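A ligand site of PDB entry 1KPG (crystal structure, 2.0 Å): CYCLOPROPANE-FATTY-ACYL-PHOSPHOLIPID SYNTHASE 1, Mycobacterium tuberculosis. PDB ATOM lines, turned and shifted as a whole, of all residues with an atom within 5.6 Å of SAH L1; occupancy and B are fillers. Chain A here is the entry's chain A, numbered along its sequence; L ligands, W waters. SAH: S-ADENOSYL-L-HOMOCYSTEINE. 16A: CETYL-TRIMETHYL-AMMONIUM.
A sulfur (SD) of SAH L1 lies close to the side-chain hydroxyl of Tyr 16, at 3.5 Å.
N of Leu 95 sits at hydrogen-bond distance from O2' of SAH L1 (3.2 Å).
The backbone NH (N) of Gly 74 lies within hydrogen-bond range of an oxygen (O3') of SAH L1, 3.2 Å away.
N of SAH L1 is in hydrogen-bond range of O of Ile 136.
A nitrogen (N6) of SAH L1 is in hydrogen-bond range of the side-chain carboxylate (OE2) of Glu 124.
A nitrogen (N) of SAH L1 sits at hydrogen-bond distance from the backbone carbonyl oxygen (O) of Gly 72 (2.6 Å).
An oxygen (O2') of SAH L1 lies within hydrogen-bond range of the side-chain hydroxyl (OG1) of Thr 94 (3.0 Å).
A nitrogen (N1) of SAH L1 sits at hydrogen-bond distance from the backbone NH of Trp 123.
The side-chain hydroxyl of Ser 34 lies within hydrogen-bond range of an oxygen (O) of SAH L1.
The backbone NH (N) of Tyr 33 sits at hydrogen-bond distance from an oxygen (OXT) of SAH L1.
The side-chain amide oxygen (OE1) of Gln 99 lies within hydrogen-bond range of an oxygen (O3') of SAH L1 (2.7 Å).
The backbone carbonyl oxygen (O) of Leu 93 lies within hydrogen-bond range of the backbone NH (N) of Cys 73 (3.0 Å).
N of Gly 72 lies within hydrogen-bond range of O of Leu 93, 2.8 Å away.
N of Leu 93 lies within hydrogen-bond range of O of Asp 70.
OE1 of Gln 99 is in hydrogen-bond range of OG1 of Thr 94, 2.8 Å away.
The backbone NH of Ala 121 sits at hydrogen-bond distance from the backbone carbonyl oxygen of Thr 94, 3.0 Å away.
The side-chain hydroxyl of Ser 96 is in hydrogen-bond range of the backbone NH of Gln 99 (3.2 Å).
OG1 of Thr 94 lies within hydrogen-bond range of N of Ser 96.
OH of Tyr 16 lies within hydrogen-bond range of NE2 of His 141, 2.6 Å away.
Val 12 touches SAH L1 (CG1 to O2', 3.4 Å).
Thr 32 touches SAH L1.
C of Cys 73 touches CA of SAH L1, at 3.9 Å.
Leu 93 touches SAH L1 (O to N3, 3.6 Å).
Ser 96 touches SAH L1 (N to O2', 3.8 Å).
Ala 121 touches SAH L1 (O to C2, 3.8 Å).
Gly 122 touches SAH L1.
Gly 137 touches SAH L1 (O to C5', 3.3 Å).
Ala 138 touches SAH L1.
His 141 touches SAH L1 (CB to C8, 3.5 Å).
Phe 142 touches SAH L1.
The nearest printed residue that does not touch SAH L1 is Gln 31 (4.3 Å).
Water W5 lies within hydrogen-bond range of the backbone carbonyl oxygen (O) of Gln 31 (2.7 Å), an oxygen (OXT) of SAH L1 (2.7 Å) and the backbone NH (N) of Trp 75 (2.9 Å).
Water W7 bridges a nitrogen (N7) of SAH L1 (2.8 Å) and the backbone carbonyl oxygen (O) of His 141 (2.9 Å).
Water W3 lies within hydrogen-bond range of a nitrogen (N) of SAH L1, the side-chain hydroxyl (OG1) of Thr 78 and the side-chain carboxylate (OD2) of Asp 70.
Water W2 bridges the side-chain hydroxyl (OG1) of Thr 78 (2.9 Å) and an oxygen (O) of SAH L1 (2.9 Å).
Water W4 lies within hydrogen-bond range of the side-chain carboxylate of Glu 124 and a nitrogen (N6) of SAH L1.
Water W6 lies within hydrogen-bond range of OE1 of Glu 124 (2.6 Å), NE1 of Trp 123 (3.1 Å) and N6 of SAH L1 (3.3 Å).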
ATOM      1  N   PRO A   7      17.863 -25.430  28.861  1.00  0.00           N
ATOM      2  CA  PRO A   7      17.255 -26.161  27.752  1.00  0.00           C
ATOM      3  C   PRO A   7      16.678 -27.490  28.231  1.00  0.00           C
ATOM      4  O   PRO A   7      17.213 -28.114  29.155  1.00  0.00           O
ATOM      5  CB  PRO A   7      18.426 -26.357  26.794  1.00  0.00           C
ATOM      6  CG  PRO A   7      19.239 -25.119  27.019  1.00  0.00           C
ATOM      7  CD  PRO A   7      19.235 -25.005  28.530  1.00  0.00           C
ATOM      8  N   VAL A  12      13.606 -33.551  24.764  1.00  0.00           N
ATOM      9  CA  VAL A  12      13.953 -33.645  23.346  1.00  0.00           C
ATOM     10  C   VAL A  12      14.733 -34.907  23.022  1.00  0.00           C
ATOM     11  O   VAL A  12      14.453 -35.582  22.037  1.00  0.00           O
ATOM     12  CB  VAL A  12      14.752 -32.411  22.907  1.00  0.00           C
ATOM     13  CG1 VAL A  12      15.262 -32.570  21.482  1.00  0.00           C
ATOM     14  CG2 VAL A  12      13.873 -31.182  23.016  1.00  0.00           C
ATOM     15  N   TYR A  16      14.554 -37.840  19.827  1.00  0.00           N
ATOM     16  CA  TYR A  16      15.658 -37.871  18.871  1.00  0.00           C
ATOM     17  C   TYR A  16      16.879 -38.744  19.156  1.00  0.00           C
ATOM     18  O   TYR A  16      17.592 -39.119  18.228  1.00  0.00           O
ATOM     19  CB  TYR A  16      16.117 -36.438  18.536  1.00  0.00           C
ATOM     20  CG  TYR A  16      14.957 -35.556  18.129  1.00  0.00           C
ATOM     21  CD1 TYR A  16      14.377 -34.656  19.035  1.00  0.00           C
ATOM     22  CD2 TYR A  16      14.374 -35.675  16.866  1.00  0.00           C
ATOM     23  CE1 TYR A  16      13.246 -33.931  18.708  1.00  0.00           C
ATOM     24  CE2 TYR A  16      13.231 -34.943  16.525  1.00  0.00           C
ATOM     25  CZ  TYR A  16      12.675 -34.078  17.450  1.00  0.00           C
ATOM     26  OH  TYR A  16      11.521 -33.380  17.143  1.00  0.00           O
ATOM     27  N   GLN A  31      18.065 -37.629   6.032  1.00  0.00           N
ATOM     28  CA  GLN A  31      17.609 -37.669   7.423  1.00  0.00           C
ATOM     29  C   GLN A  31      16.816 -36.423   7.807  1.00  0.00           C
ATOM     30  O   GLN A  31      16.785 -36.044   8.991  1.00  0.00           O
ATOM     31  CB  GLN A  31      18.799 -37.829   8.389  1.00  0.00           C
ATOM     32  CG  GLN A  31      19.653 -39.077   8.163  1.00  0.00           C
ATOM     33  CD  GLN A  31      18.813 -40.305   7.866  1.00  0.00           C
ATOM     34  OE1 GLN A  31      18.847 -40.847   6.755  1.00  0.00           O
ATOM     35  NE2 GLN A  31      18.048 -40.757   8.862  1.00  0.00           N
ATOM     36  N   THR A  32      16.191 -35.778   6.816  1.00  0.00           N
ATOM     37  CA  THR A  32      15.383 -34.588   7.099  1.00  0.00           C
ATOM     38  C   THR A  32      14.128 -35.086   7.819  1.00  0.00           C
ATOM     39  O   THR A  32      13.436 -35.975   7.321  1.00  0.00           O
ATOM     40  CB  THR A  32      14.996 -33.841   5.790  1.00  0.00           C
ATOM     41  OG1 THR A  32      16.185 -33.348   5.155  1.00  0.00           O
ATOM     42  CG2 THR A  32      14.088 -32.653   6.090  1.00  0.00           C
ATOM     43  N   TYR A  33      13.857 -34.512   8.986  1.00  0.00           N
ATOM     44  CA  TYR A  33      12.728 -34.932   9.821  1.00  0.00           C
ATOM     45  C   TYR A  33      11.728 -33.786   9.966  1.00  0.00           C
ATOM     46  O   TYR A  33      11.535 -33.234  11.052  1.00  0.00           O
ATOM     47  CB  TYR A  33      13.275 -35.351  11.199  1.00  0.00           C
ATOM     48  CG  TYR A  33      12.364 -36.198  12.064  1.00  0.00           C
ATOM     49  CD1 TYR A  33      11.105 -36.628  11.618  1.00  0.00           C
ATOM     50  CD2 TYR A  33      12.768 -36.587  13.341  1.00  0.00           C
ATOM     51  CE1 TYR A  33      10.284 -37.419  12.418  1.00  0.00           C
ATOM     52  CE2 TYR A  33      11.943 -37.381  14.157  1.00  0.00           C
ATOM     53  CZ  TYR A  33      10.710 -37.790  13.684  1.00  0.00           C
ATOM     54  OH  TYR A  33       9.893 -38.579  14.467  1.00  0.00           O
ATOM     55  N   SER A  34      11.102 -33.429   8.842  1.00  0.00           N
ATOM     56  CA  SER A  34      10.129 -32.355   8.797  1.00  0.00           C
ATOM     57  C   SER A  34       9.352 -32.448   7.491  1.00  0.00           C
ATOM     58  O   SER A  34       9.641 -33.288   6.631  1.00  0.00           O
ATOM     59  CB  SER A  34      10.836 -31.009   8.929  1.00  0.00           C
ATOM     60  OG  SER A  34      11.967 -30.934   8.073  1.00  0.00           O
ATOM     61  N   LYS A  52      12.104 -28.484  -0.075  1.00  0.00           N
ATOM     62  CA  LYS A  52      11.668 -27.789   1.130  1.00  0.00           C
ATOM     63  C   LYS A  52      12.846 -26.991   1.708  1.00  0.00           C
ATOM     64  O   LYS A  52      12.670 -25.863   2.170  1.00  0.00           O
ATOM     65  CB  LYS A  52      11.115 -28.794   2.154  1.00  0.00           C
ATOM     66  CG  LYS A  52      10.741 -28.197   3.498  1.00  0.00           C
ATOM     67  CD  LYS A  52      11.932 -28.114   4.428  1.00  0.00           C
ATOM     68  CE  LYS A  52      12.524 -29.491   4.744  1.00  0.00           C
ATOM     69  NZ  LYS A  52      11.535 -30.421   5.350  1.00  0.00           N
ATOM     70  N   ASP A  70      21.189 -22.354  12.310  1.00  0.00           N
ATOM     71  CA  ASP A  70      20.124 -23.336  12.182  1.00  0.00           C
ATOM     72  C   ASP A  70      19.722 -23.777  13.591  1.00  0.00           C
ATOM     73  O   ASP A  70      20.456 -24.526  14.246  1.00  0.00           O
ATOM     74  CB  ASP A  70      20.573 -24.567  11.381  1.00  0.00           C
ATOM     75  CG  ASP A  70      19.421 -25.505  11.052  1.00  0.00           C
ATOM     76  OD1 ASP A  70      18.379 -25.439  11.728  1.00  0.00           O
ATOM     77  OD2 ASP A  70      19.547 -26.312  10.110  1.00  0.00           O
ATOM     78  N   VAL A  71      18.576 -23.299  14.040  1.00  0.00           N
ATOM     79  CA  VAL A  71      18.079 -23.649  15.380  1.00  0.00           C
ATOM     80  C   VAL A  71      17.284 -24.947  15.294  1.00  0.00           C
ATOM     81  O   VAL A  71      16.172 -24.966  14.771  1.00  0.00           O
ATOM     82  CB  VAL A  71      17.184 -22.527  15.950  1.00  0.00           C
ATOM     83  CG1 VAL A  71      16.619 -22.934  17.307  1.00  0.00           C
ATOM     84  CG2 VAL A  71      17.987 -21.248  16.077  1.00  0.00           C
ATOM     85  N   GLY A  72      17.875 -26.024  15.823  1.00  0.00           N
ATOM     86  CA  GLY A  72      17.242 -27.330  15.775  1.00  0.00           C
ATOM     87  C   GLY A  72      17.661 -27.989  14.475  1.00  0.00           C
ATOM     88  O   GLY A  72      16.828 -28.409  13.683  1.00  0.00           O
ATOM     89  N   CYS A  73      18.968 -28.080  14.267  1.00  0.00           N
ATOM     90  CA  CYS A  73      19.548 -28.616  13.031  1.00  0.00           C
ATOM     91  C   CYS A  73      19.321 -30.075  12.686  1.00  0.00           C
ATOM     92  O   CYS A  73      19.686 -30.517  11.604  1.00  0.00           O
ATOM     93  CB  CYS A  73      21.049 -28.314  12.995  1.00  0.00           C
ATOM     94  SG  CYS A  73      22.036 -29.154  14.266  1.00  0.00           S
ATOM     95  N   GLY A  74      18.726 -30.843  13.598  1.00  0.00           N
ATOM     96  CA  GLY A  74      18.484 -32.246  13.324  1.00  0.00           C
ATOM     97  C   GLY A  74      19.757 -32.941  12.880  1.00  0.00           C
ATOM     98  O   GLY A  74      20.820 -32.709  13.471  1.00  0.00           O
ATOM     99  N   TRP A  75      19.666 -33.781  11.856  1.00  0.00           N
ATOM    100  CA  TRP A  75      20.839 -34.500  11.360  1.00  0.00           C
ATOM    101  C   TRP A  75      21.688 -33.734  10.335  1.00  0.00           C
ATOM    102  O   TRP A  75      22.447 -34.332   9.553  1.00  0.00           O
ATOM    103  CB  TRP A  75      20.419 -35.874  10.843  1.00  0.00           C
ATOM    104  CG  TRP A  75      20.100 -36.802  11.972  1.00  0.00           C
ATOM    105  CD1 TRP A  75      20.994 -37.461  12.774  1.00  0.00           C
ATOM    106  CD2 TRP A  75      18.800 -37.127  12.491  1.00  0.00           C
ATOM    107  NE1 TRP A  75      20.334 -38.169  13.745  1.00  0.00           N
ATOM    108  CE2 TRP A  75      18.991 -37.980  13.605  1.00  0.00           C
ATOM    109  CE3 TRP A  75      17.489 -36.774  12.119  1.00  0.00           C
ATOM    110  CZ2 TRP A  75      17.918 -38.497  14.354  1.00  0.00           C
ATOM    111  CZ3 TRP A  75      16.430 -37.279  12.862  1.00  0.00           C
ATOM    112  CH2 TRP A  75      16.655 -38.142  13.970  1.00  0.00           C
ATOM    113  N   THR A  78      20.062 -29.442   6.268  1.00  0.00           N
ATOM    114  CA  THR A  78      19.875 -28.035   5.922  1.00  0.00           C
ATOM    115  C   THR A  78      21.175 -27.236   5.990  1.00  0.00           C
ATOM    116  O   THR A  78      21.471 -26.435   5.119  1.00  0.00           O
ATOM    117  CB  THR A  78      18.809 -27.377   6.837  1.00  0.00           C
ATOM    118  OG1 THR A  78      17.552 -28.017   6.612  1.00  0.00           O
ATOM    119  CG2 THR A  78      18.653 -25.884   6.536  1.00  0.00           C
ATOM    120  N   LEU A  93      22.382 -25.739  16.067  1.00  0.00           N
ATOM    121  CA  LEU A  93      22.088 -26.031  17.470  1.00  0.00           C
ATOM    122  C   LEU A  93      21.113 -27.202  17.582  1.00  0.00           C
ATOM    123  O   LEU A  93      20.120 -27.260  16.859  1.00  0.00           O
ATOM    124  CB  LEU A  93      21.476 -24.800  18.131  1.00  0.00           C
ATOM    125  CG  LEU A  93      22.358 -23.654  18.635  1.00  0.00           C
ATOM    126  CD1 LEU A  93      23.605 -23.498  17.789  1.00  0.00           C
ATOM    127  CD2 LEU A  93      21.528 -22.368  18.656  1.00  0.00           C
ATOM    128  N   THR A  94      21.392 -28.122  18.496  1.00  0.00           N
ATOM    129  CA  THR A  94      20.515 -29.277  18.730  1.00  0.00           C
ATOM    130  C   THR A  94      20.667 -29.762  20.153  1.00  0.00           C
ATOM    131  O   THR A  94      21.736 -29.617  20.751  1.00  0.00           O
ATOM    132  CB  THR A  94      20.841 -30.452  17.793  1.00  0.00           C
ATOM    133  OG1 THR A  94      19.910 -31.522  18.032  1.00  0.00           O
ATOM    134  CG2 THR A  94      22.262 -30.961  18.030  1.00  0.00           C
ATOM    135  N   LEU A  95      19.599 -30.323  20.717  1.00  0.00           N
ATOM    136  CA  LEU A  95      19.638 -30.835  22.084  1.00  0.00           C
ATOM    137  C   LEU A  95      19.869 -32.338  22.054  1.00  0.00           C
ATOM    138  O   LEU A  95      19.985 -32.970  23.104  1.00  0.00           O
ATOM    139  CB  LEU A  95      18.331 -30.516  22.825  1.00  0.00           C
ATOM    140  CG  LEU A  95      17.941 -29.042  22.938  1.00  0.00           C
ATOM    141  CD1 LEU A  95      16.730 -28.901  23.861  1.00  0.00           C
ATOM    142  CD2 LEU A  95      19.106 -28.236  23.503  1.00  0.00           C
ATOM    143  N   SER A  96      19.925 -32.894  20.844  1.00  0.00           N
ATOM    144  CA  SER A  96      20.134 -34.324  20.657  1.00  0.00           C
ATOM    145  C   SER A  96      21.610 -34.701  20.567  1.00  0.00           C
ATOM    146  O   SER A  96      22.355 -34.134  19.764  1.00  0.00           O
ATOM    147  CB  SER A  96      19.410 -34.781  19.375  1.00  0.00           C
ATOM    148  OG  SER A  96      19.828 -36.080  18.982  1.00  0.00           O
ATOM    149  N   GLN A  99      22.350 -36.556  17.150  1.00  0.00           N
ATOM    150  CA  GLN A  99      22.381 -35.643  15.997  1.00  0.00           C
ATOM    151  C   GLN A  99      23.656 -34.793  16.042  1.00  0.00           C
ATOM    152  O   GLN A  99      24.292 -34.567  15.018  1.00  0.00           O
ATOM    153  CB  GLN A  99      21.151 -34.723  15.988  1.00  0.00           C
ATOM    154  CG  GLN A  99      19.820 -35.468  15.861  1.00  0.00           C
ATOM    155  CD  GLN A  99      18.626 -34.541  15.908  1.00  0.00           C
ATOM    156  OE1 GLN A  99      18.699 -33.445  16.462  1.00  0.00           O
ATOM    157  NE2 GLN A  99      17.499 -34.995  15.346  1.00  0.00           N
ATOM    158  N   ALA A 121      23.593 -27.734  22.183  1.00  0.00           N
ATOM    159  CA  ALA A 121      23.138 -26.629  23.013  1.00  0.00           C
ATOM    160  C   ALA A 121      21.842 -26.060  22.466  1.00  0.00           C
ATOM    161  O   ALA A 121      21.528 -26.223  21.286  1.00  0.00           O
ATOM    162  CB  ALA A 121      24.220 -25.545  23.034  1.00  0.00           C
ATOM    163  N   GLY A 122      21.075 -25.399  23.316  1.00  0.00           N
ATOM    164  CA  GLY A 122      19.838 -24.821  22.851  1.00  0.00           C
ATOM    165  C   GLY A 122      20.065 -23.375  22.486  1.00  0.00           C
ATOM    166  O   GLY A 122      21.110 -22.799  22.824  1.00  0.00           O
ATOM    167  N   TRP A 123      19.103 -22.779  21.784  1.00  0.00           N
ATOM    168  CA  TRP A 123      19.237 -21.376  21.438  1.00  0.00           C
ATOM    169  C   TRP A 123      19.369 -20.586  22.728  1.00  0.00           C
ATOM    170  O   TRP A 123      19.938 -19.488  22.741  1.00  0.00           O
ATOM    171  CB  TRP A 123      18.002 -20.888  20.666  1.00  0.00           C
ATOM    172  CG  TRP A 123      16.683 -21.173  21.337  1.00  0.00           C
ATOM    173  CD1 TRP A 123      15.868 -22.253  21.122  1.00  0.00           C
ATOM    174  CD2 TRP A 123      16.005 -20.354  22.303  1.00  0.00           C
ATOM    175  NE1 TRP A 123      14.735 -22.156  21.895  1.00  0.00           N
ATOM    176  CE2 TRP A 123      14.801 -20.999  22.630  1.00  0.00           C
ATOM    177  CE3 TRP A 123      16.313 -19.135  22.926  1.00  0.00           C
ATOM    178  CZ2 TRP A 123      13.883 -20.466  23.550  1.00  0.00           C
ATOM    179  CZ3 TRP A 123      15.412 -18.606  23.843  1.00  0.00           C
ATOM    180  CH2 TRP A 123      14.217 -19.273  24.151  1.00  0.00           C
ATOM    181  N   GLU A 124      18.860 -21.158  23.822  1.00  0.00           N
ATOM    182  CA  GLU A 124      18.899 -20.541  25.136  1.00  0.00           C
ATOM    183  C   GLU A 124      20.320 -20.260  25.605  1.00  0.00           C
ATOM    184  O   GLU A 124      20.531 -19.463  26.514  1.00  0.00           O
ATOM    185  CB  GLU A 124      18.242 -21.457  26.185  1.00  0.00           C
ATOM    186  CG  GLU A 124      16.730 -21.646  26.073  1.00  0.00           C
ATOM    187  CD  GLU A 124      16.332 -22.852  25.251  1.00  0.00           C
ATOM    188  OE1 GLU A 124      15.208 -23.360  25.461  1.00  0.00           O
ATOM    189  OE2 GLU A 124      17.121 -23.297  24.390  1.00  0.00           O
ATOM    190  N   SER A 135      14.928 -22.121  11.155  1.00  0.00           N
ATOM    191  CA  SER A 135      14.520 -23.067  12.182  1.00  0.00           C
ATOM    192  C   SER A 135      13.330 -23.836  11.629  1.00  0.00           C
ATOM    193  O   SER A 135      12.272 -23.268  11.386  1.00  0.00           O
ATOM    194  CB  SER A 135      14.133 -22.333  13.477  1.00  0.00           C
ATOM    195  OG  SER A 135      13.804 -23.257  14.501  1.00  0.00           O
ATOM    196  N   ILE A 136      13.511 -25.141  11.430  1.00  0.00           N
ATOM    197  CA  ILE A 136      12.464 -25.975  10.860  1.00  0.00           C
ATOM    198  C   ILE A 136      12.070 -27.139  11.792  1.00  0.00           C
ATOM    199  O   ILE A 136      12.872 -28.050  12.030  1.00  0.00           O
ATOM    200  CB  ILE A 136      12.922 -26.529   9.508  1.00  0.00           C
ATOM    201  CG1 ILE A 136      13.226 -25.370   8.554  1.00  0.00           C
ATOM    202  CG2 ILE A 136      11.881 -27.471   8.935  1.00  0.00           C
ATOM    203  CD1 ILE A 136      14.095 -25.739   7.347  1.00  0.00           C
ATOM    204  N   GLY A 137      10.848 -27.077  12.310  1.00  0.00           N
ATOM    205  CA  GLY A 137      10.357 -28.122  13.188  1.00  0.00           C
ATOM    206  C   GLY A 137      10.927 -28.200  14.604  1.00  0.00           C
ATOM    207  O   GLY A 137      10.811 -29.244  15.249  1.00  0.00           O
ATOM    208  N   ALA A 138      11.530 -27.129  15.090  1.00  0.00           N
ATOM    209  CA  ALA A 138      12.092 -27.115  16.446  1.00  0.00           C
ATOM    210  C   ALA A 138      11.222 -26.276  17.393  1.00  0.00           C
ATOM    211  O   ALA A 138      11.128 -26.557  18.595  1.00  0.00           O
ATOM    212  CB  ALA A 138      13.508 -26.559  16.415  1.00  0.00           C
ATOM    213  N   HIS A 141       9.008 -27.553  20.191  1.00  0.00           N
ATOM    214  CA  HIS A 141       9.615 -28.070  21.407  1.00  0.00           C
ATOM    215  C   HIS A 141       9.934 -26.959  22.424  1.00  0.00           C
ATOM    216  O   HIS A 141      10.270 -27.236  23.574  1.00  0.00           O
ATOM    217  CB  HIS A 141      10.923 -28.793  21.075  1.00  0.00           C
ATOM    218  CG  HIS A 141      10.739 -30.123  20.400  1.00  0.00           C
ATOM    219  ND1 HIS A 141      10.287 -31.231  21.067  1.00  0.00           N
ATOM    220  CD2 HIS A 141      10.989 -30.515  19.129  1.00  0.00           C
ATOM    221  CE1 HIS A 141      10.266 -32.260  20.242  1.00  0.00           C
ATOM    222  NE2 HIS A 141      10.682 -31.859  19.058  1.00  0.00           N
ATOM    223  N   PHE A 142       9.837 -25.712  21.987  1.00  0.00           N
ATOM    224  CA  PHE A 142      10.160 -24.596  22.874  1.00  0.00           C
ATOM    225  C   PHE A 142       9.200 -24.439  24.039  1.00  0.00           C
ATOM    226  O   PHE A 142       9.622 -24.159  25.156  1.00  0.00           O
ATOM    227  CB  PHE A 142      10.227 -23.287  22.065  1.00  0.00           C
ATOM    228  CG  PHE A 142      11.259 -23.304  20.949  1.00  0.00           C
ATOM    229  CD1 PHE A 142      12.158 -24.368  20.822  1.00  0.00           C
ATOM    230  CD2 PHE A 142      11.340 -22.250  20.040  1.00  0.00           C
ATOM    231  CE1 PHE A 142      13.128 -24.367  19.814  1.00  0.00           C
ATOM    232  CE2 PHE A 142      12.311 -22.239  19.022  1.00  0.00           C
ATOM    233  CZ  PHE A 142      13.206 -23.306  18.911  1.00  0.00           C
HETATM  234  N   SAH L   1      15.426 -28.988  11.553  1.00  0.00           N
HETATM  235  CA  SAH L   1      15.673 -30.420  11.387  1.00  0.00           C
HETATM  236  CB  SAH L   1      15.312 -31.227  12.643  1.00  0.00           C
HETATM  237  CG  SAH L   1      13.855 -31.145  13.167  1.00  0.00           C
HETATM  238  SD  SAH L   1      13.554 -32.177  14.627  1.00  0.00           S
HETATM  239  C   SAH L   1      14.886 -30.983  10.194  1.00  0.00           C
HETATM  240  O   SAH L   1      13.951 -30.283   9.736  1.00  0.00           O
HETATM  241  OXT SAH L   1      15.191 -32.111   9.745  1.00  0.00           O
HETATM  242  C5' SAH L   1      13.475 -30.969  15.977  1.00  0.00           C
HETATM  243  C4' SAH L   1      14.866 -30.398  16.249  1.00  0.00           C
HETATM  244  O4' SAH L   1      14.881 -29.188  17.057  1.00  0.00           O
HETATM  245  C3' SAH L   1      15.807 -31.378  16.930  1.00  0.00           C
HETATM  246  O3' SAH L   1      17.082 -31.328  16.249  1.00  0.00           O
HETATM  247  C2' SAH L   1      15.900 -30.849  18.352  1.00  0.00           C
HETATM  248  O2' SAH L   1      17.093 -31.278  18.990  1.00  0.00           O
HETATM  249  C1' SAH L   1      15.838 -29.384  18.111  1.00  0.00           C
HETATM  250  N9  SAH L   1      15.502 -28.548  19.284  1.00  0.00           N
HETATM  251  C8  SAH L   1      14.313 -28.576  20.186  1.00  0.00           C
HETATM  252  N7  SAH L   1      14.329 -27.693  21.126  1.00  0.00           N
HETATM  253  C5  SAH L   1      15.551 -26.999  20.895  1.00  0.00           C
HETATM  254  C6  SAH L   1      16.173 -25.899  21.564  1.00  0.00           C
HETATM  255  N6  SAH L   1      15.617 -25.287  22.631  1.00  0.00           N
HETATM  256  N1  SAH L   1      17.378 -25.440  21.083  1.00  0.00           N
HETATM  257  C2  SAH L   1      17.935 -26.042  20.006  1.00  0.00           C
HETATM  258  N3  SAH L   1      17.459 -27.074  19.298  1.00  0.00           N
HETATM  259  C4  SAH L   1      16.255 -27.513  19.788  1.00  0.00           C
HETATM  260  C1  16A L   2       4.742 -34.736  12.337  1.00  0.00           C
HETATM  261  C2  16A L   2       4.399 -34.265  13.759  1.00  0.00           C
HETATM  262  C3  16A L   2       2.946 -33.757  13.837  1.00  0.00           C
HETATM  263  C4  16A L   2       2.506 -33.260  15.216  1.00  0.00           C
HETATM  264  C5  16A L   2       1.037 -32.790  15.189  1.00  0.00           C
HETATM  265  C6  16A L   2       0.474 -32.252  16.525  1.00  0.00           C
HETATM  266  C7  16A L   2       0.613 -33.065  17.836  1.00  0.00           C
HETATM  267  C8  16A L   2       1.397 -32.531  19.060  1.00  0.00           C
HETATM  268  C9  16A L   2       1.785 -31.031  19.168  1.00  0.00           C
HETATM  269  C10 16A L   2       3.173 -30.696  18.647  1.00  0.00           C
HETATM  270  C11 16A L   2       4.391 -30.832  19.599  1.00  0.00           C
HETATM  271  C12 16A L   2       5.687 -31.546  19.140  1.00  0.00           C
HETATM  272  C13 16A L   2       6.108 -31.382  17.657  1.00  0.00           C
HETATM  273  C14 16A L   2       7.390 -32.112  17.288  1.00  0.00           C
HETATM  274  C15 16A L   2       7.553 -32.061  15.763  1.00  0.00           C
HETATM  275  C16 16A L   2       8.801 -32.871  15.325  1.00  0.00           C
HETATM  276  N1  16A L   2       9.264 -33.012  13.951  1.00  0.00           N
HETATM  277  C17 16A L   2      10.464 -33.923  14.064  1.00  0.00           C
HETATM  278  C18 16A L   2       8.280 -33.682  13.007  1.00  0.00           C
HETATM  279  C19 16A L   2       9.781 -31.700  13.402  1.00  0.00           C
HETATM  280  O   HOH W   1      15.909 -26.183  12.100  1.00  0.00           O
HETATM  281  O   HOH W   2      15.013 -29.235   7.232  1.00  0.00           O
HETATM  282  O   HOH W   3      17.105 -27.929   9.536  1.00  0.00           O
HETATM  283  O   HOH W   4      14.591 -26.141  25.533  1.00  0.00           O
HETATM  284  O   HOH W   5      17.288 -33.707  10.170  1.00  0.00           O
HETATM  285  O   HOH W   6      13.081 -23.728  24.028  1.00  0.00           O
HETATM  286  O   HOH W   7      13.216 -27.206  23.631  1.00  0.00           O
